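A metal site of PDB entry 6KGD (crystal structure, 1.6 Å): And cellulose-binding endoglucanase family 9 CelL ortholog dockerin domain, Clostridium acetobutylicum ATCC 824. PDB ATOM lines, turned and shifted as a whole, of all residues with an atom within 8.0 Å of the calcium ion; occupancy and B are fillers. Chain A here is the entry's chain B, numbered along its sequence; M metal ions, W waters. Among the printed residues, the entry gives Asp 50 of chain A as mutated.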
ATOM      1  N   MET A  22      12.774  25.909 -24.602  1.00  0.00           N
ATOM      2  CA  MET A  22      12.464  24.586 -24.101  1.00  0.00           C
ATOM      3  C   MET A  22      12.217  23.602 -25.240  1.00  0.00           C
ATOM      4  O   MET A  22      12.674  22.459 -25.199  1.00  0.00           O
ATOM      5  CB  MET A  22      11.247  24.641 -23.187  1.00  0.00           C
ATOM      6  CG  MET A  22      10.771  23.267 -22.695  1.00  0.00           C
ATOM      7  SD  MET A  22      11.883  22.500 -21.513  1.00  0.00           S
ATOM      8  CE  MET A  22      11.320  23.278 -19.991  1.00  0.00           C
ATOM      9  N   LEU A  39      15.237  24.464 -16.118  1.00  0.00           N
ATOM     10  CA  LEU A  39      14.603  23.557 -17.064  1.00  0.00           C
ATOM     11  C   LEU A  39      13.655  22.569 -16.383  1.00  0.00           C
ATOM     12  O   LEU A  39      12.579  22.265 -16.908  1.00  0.00           O
ATOM     13  CB  LEU A  39      15.661  22.770 -17.835  1.00  0.00           C
ATOM     14  CG  LEU A  39      16.412  23.495 -18.940  1.00  0.00           C
ATOM     15  CD1 LEU A  39      17.551  22.607 -19.419  1.00  0.00           C
ATOM     16  CD2 LEU A  39      15.484  23.793 -20.081  1.00  0.00           C
ATOM     17  N   ASP A  40      14.050  22.037 -15.222  1.00  0.00           N
ATOM     18  CA  ASP A  40      13.245  21.026 -14.539  1.00  0.00           C
ATOM     19  C   ASP A  40      12.179  21.729 -13.696  1.00  0.00           C
ATOM     20  O   ASP A  40      12.262  21.830 -12.468  1.00  0.00           O
ATOM     21  CB  ASP A  40      14.131  20.124 -13.709  1.00  0.00           C
ATOM     22  CG  ASP A  40      13.364  19.034 -13.008  1.00  0.00           C
ATOM     23  OD1 ASP A  40      12.199  18.790 -13.408  1.00  0.00           O
ATOM     24  OD2 ASP A  40      13.937  18.416 -12.065  1.00  0.00           O
ATOM     25  N   ILE A  41      11.160  22.227 -14.391  1.00  0.00           N
ATOM     26  CA  ILE A  41      10.176  23.086 -13.748  1.00  0.00           C
ATOM     27  C   ILE A  41       9.398  22.370 -12.647  1.00  0.00           C
ATOM     28  O   ILE A  41       9.023  22.983 -11.644  1.00  0.00           O
ATOM     29  CB  ILE A  41       9.237  23.670 -14.829  1.00  0.00           C
ATOM     30  CG1 ILE A  41      10.073  24.543 -15.770  1.00  0.00           C
ATOM     31  CG2 ILE A  41       8.090  24.421 -14.197  1.00  0.00           C
ATOM     32  CD1 ILE A  41       9.297  25.081 -16.947  1.00  0.00           C
ATOM     33  N   ASN A  42       9.124  21.077 -12.822  1.00  0.00           N
ATOM     34  CA  ASN A  42       8.358  20.364 -11.796  1.00  0.00           C
ATOM     35  C   ASN A  42       9.254  19.635 -10.794  1.00  0.00           C
ATOM     36  O   ASN A  42       8.739  19.029  -9.849  1.00  0.00           O
ATOM     37  CB  ASN A  42       7.363  19.379 -12.463  1.00  0.00           C
ATOM     38  CG  ASN A  42       8.047  18.360 -13.358  1.00  0.00           C
ATOM     39  OD1 ASN A  42       9.228  18.085 -13.212  1.00  0.00           O
ATOM     40  ND2 ASN A  42       7.287  17.789 -14.276  1.00  0.00           N
ATOM     41  N   GLY A  43      10.572  19.706 -10.953  1.00  0.00           N
ATOM     42  CA  GLY A  43      11.480  19.195  -9.951  1.00  0.00           C
ATOM     43  C   GLY A  43      11.507  17.692  -9.789  1.00  0.00           C
ATOM     44  O   GLY A  43      11.875  17.197  -8.716  1.00  0.00           O
ATOM     45  N   ASP A  44      11.138  16.934 -10.820  1.00  0.00           N
ATOM     46  CA  ASP A  44      11.146  15.479 -10.729  1.00  0.00           C
ATOM     47  C   ASP A  44      12.455  14.877 -11.206  1.00  0.00           C
ATOM     48  O   ASP A  44      12.541  13.653 -11.330  1.00  0.00           O
ATOM     49  CB  ASP A  44       9.974  14.876 -11.523  1.00  0.00           C
ATOM     50  CG  ASP A  44      10.098  15.097 -13.025  1.00  0.00           C
ATOM     51  OD1 ASP A  44      11.073  15.749 -13.472  1.00  0.00           O
ATOM     52  OD2 ASP A  44       9.206  14.597 -13.761  1.00  0.00           O
ATOM     53  N   GLY A  45      13.470  15.706 -11.480  1.00  0.00           N
ATOM     54  CA  GLY A  45      14.799  15.258 -11.851  1.00  0.00           C
ATOM     55  C   GLY A  45      15.019  15.029 -13.332  1.00  0.00           C
ATOM     56  O   GLY A  45      16.145  14.725 -13.739  1.00  0.00           O
ATOM     57  N   ALA A  46      13.973  15.137 -14.156  1.00  0.00           N
ATOM     58  CA  ALA A  46      14.107  14.941 -15.588  1.00  0.00           C
ATOM     59  C   ALA A  46      13.618  16.199 -16.273  1.00  0.00           C
ATOM     60  O   ALA A  46      12.797  16.938 -15.732  1.00  0.00           O
ATOM     61  CB  ALA A  46      13.308  13.742 -16.078  1.00  0.00           C
ATOM     62  N   VAL A  47      14.120  16.447 -17.475  1.00  0.00           N
ATOM     63  CA  VAL A  47      13.607  17.521 -18.310  1.00  0.00           C
ATOM     64  C   VAL A  47      12.900  16.864 -19.472  1.00  0.00           C
ATOM     65  O   VAL A  47      13.535  16.173 -20.270  1.00  0.00           O
ATOM     66  CB  VAL A  47      14.714  18.452 -18.817  1.00  0.00           C
ATOM     67  CG1 VAL A  47      14.090  19.580 -19.642  1.00  0.00           C
ATOM     68  CG2 VAL A  47      15.519  19.032 -17.678  1.00  0.00           C
ATOM     69  N   ASN A  48      11.587  17.078 -19.570  1.00  0.00           N
ATOM     70  CA  ASN A  48      10.793  16.384 -20.585  1.00  0.00           C
ATOM     71  C   ASN A  48       9.531  17.186 -20.884  1.00  0.00           C
ATOM     72  O   ASN A  48       9.388  18.341 -20.485  1.00  0.00           O
ATOM     73  CB  ASN A  48      10.466  14.953 -20.163  1.00  0.00           C
ATOM     74  CG  ASN A  48       9.685  14.860 -18.866  1.00  0.00           C
ATOM     75  OD1 ASN A  48       8.932  15.763 -18.516  1.00  0.00           O
ATOM     76  ND2 ASN A  48       9.867  13.751 -18.157  1.00  0.00           N
ATOM     77  N   GLY A  49       8.635  16.566 -21.653  1.00  0.00           N
ATOM     78  CA  GLY A  49       7.402  17.218 -22.080  1.00  0.00           C
ATOM     79  C   GLY A  49       6.533  17.714 -20.947  1.00  0.00           C
ATOM     80  O   GLY A  49       5.744  18.639 -21.167  1.00  0.00           O
ATOM     81  N   ASP A  50       6.644  17.133 -19.757  1.00  0.00           N
ATOM     82  CA  ASP A  50       5.855  17.620 -18.629  1.00  0.00           C
ATOM     83  C   ASP A  50       6.340  18.989 -18.176  1.00  0.00           C
ATOM     84  O   ASP A  50       5.553  19.810 -17.683  1.00  0.00           O
ATOM     85  CB  ASP A  50       5.890  16.643 -17.453  1.00  0.00           C
ATOM     86  CG  ASP A  50       5.235  15.324 -17.759  1.00  0.00           C
ATOM     87  OD1 ASP A  50       4.604  15.183 -18.833  1.00  0.00           O
ATOM     88  OD2 ASP A  50       5.347  14.408 -16.908  1.00  0.00           O
ATOM     89  N   ASP A  51       7.650  19.239 -18.282  1.00  0.00           N
ATOM     90  CA  ASP A  51       8.179  20.567 -17.972  1.00  0.00           C
ATOM     91  C   ASP A  51       7.727  21.576 -19.005  1.00  0.00           C
ATOM     92  O   ASP A  51       7.358  22.702 -18.666  1.00  0.00           O
ATOM     93  CB  ASP A  51       9.693  20.492 -17.895  1.00  0.00           C
ATOM     94  CG  ASP A  51      10.140  19.553 -16.824  1.00  0.00           C
ATOM     95  OD1 ASP A  51       9.865  19.870 -15.640  1.00  0.00           O
ATOM     96  OD2 ASP A  51      10.716  18.504 -17.171  1.00  0.00           O
ATOM     97  N   LEU A  52       7.735  21.167 -20.271  1.00  0.00           N
ATOM     98  CA  LEU A  52       7.187  22.021 -21.306  1.00  0.00           C
ATOM     99  C   LEU A  52       5.730  22.339 -21.021  1.00  0.00           C
ATOM    100  O   LEU A  52       5.302  23.493 -21.139  1.00  0.00           O
ATOM    101  CB  LEU A  52       7.342  21.357 -22.669  1.00  0.00           C
ATOM    102  CG  LEU A  52       6.677  22.120 -23.825  1.00  0.00           C
ATOM    103  CD1 LEU A  52       7.210  23.519 -24.037  1.00  0.00           C
ATOM    104  CD2 LEU A  52       6.827  21.296 -25.101  1.00  0.00           C
ATOM    105  N   GLU A  54       4.227  22.444 -18.122  1.00  0.00           N
ATOM    106  CA  GLU A  54       4.134  23.368 -17.005  1.00  0.00           C
ATOM    107  C   GLU A  54       4.474  24.791 -17.434  1.00  0.00           C
ATOM    108  O   GLU A  54       3.916  25.754 -16.897  1.00  0.00           O
ATOM    109  CB  GLU A  54       5.069  22.927 -15.878  1.00  0.00           C
ATOM    110  CG  GLU A  54       4.746  21.584 -15.286  1.00  0.00           C
ATOM    111  CD  GLU A  54       3.419  21.534 -14.573  1.00  0.00           C
ATOM    112  OE1 GLU A  54       2.804  22.608 -14.362  1.00  0.00           O
ATOM    113  OE2 GLU A  54       2.996  20.424 -14.203  1.00  0.00           O
HETATM  114 CA    CA M   1      10.863  17.710 -14.868  1.00  0.00          CA
HETATM  115  O   HOH W   1       9.204  16.197 -15.788  1.00  0.00           O
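N of Asn 48 sits close to OD2 of Asp 51 (2.9 Å).
N of Ile 41 lies close to OD1 of Asp 51 (3.0 Å).
OD2 of Asp 40 lies within hydrogen-bond range of N of Gly 45 (2.8 Å).
OD1 of Asp 40 lies close to N of Gly 43.
The calcium ion is bound by the backbone carbonyl oxygen (O) of Ala 46 (2.3 Å).
OD1 of Asp 40 is bound to the calcium ion, 2.3 Å away.
The calcium ion is bound by the side-chain amide oxygen (OD1) of Asn 42.
The calcium ion is bound by OD1 of Asp 44 (2.4 Å).
The calcium ion is bound by water W1, 2.4 Å away.
The calcium ion is bound by OD2 of Asp 51 (2.4 Å).
The calcium ion is bound by OD1 of Asp 51 (2.5 Å).
Water W1 lies within hydrogen-bond range of the side-chain carboxylate (OD2) of Asp 44, the side-chain amide oxygen (OD1) of Asn 48 and the side-chain amide nitrogen (ND2) of Asn 42.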
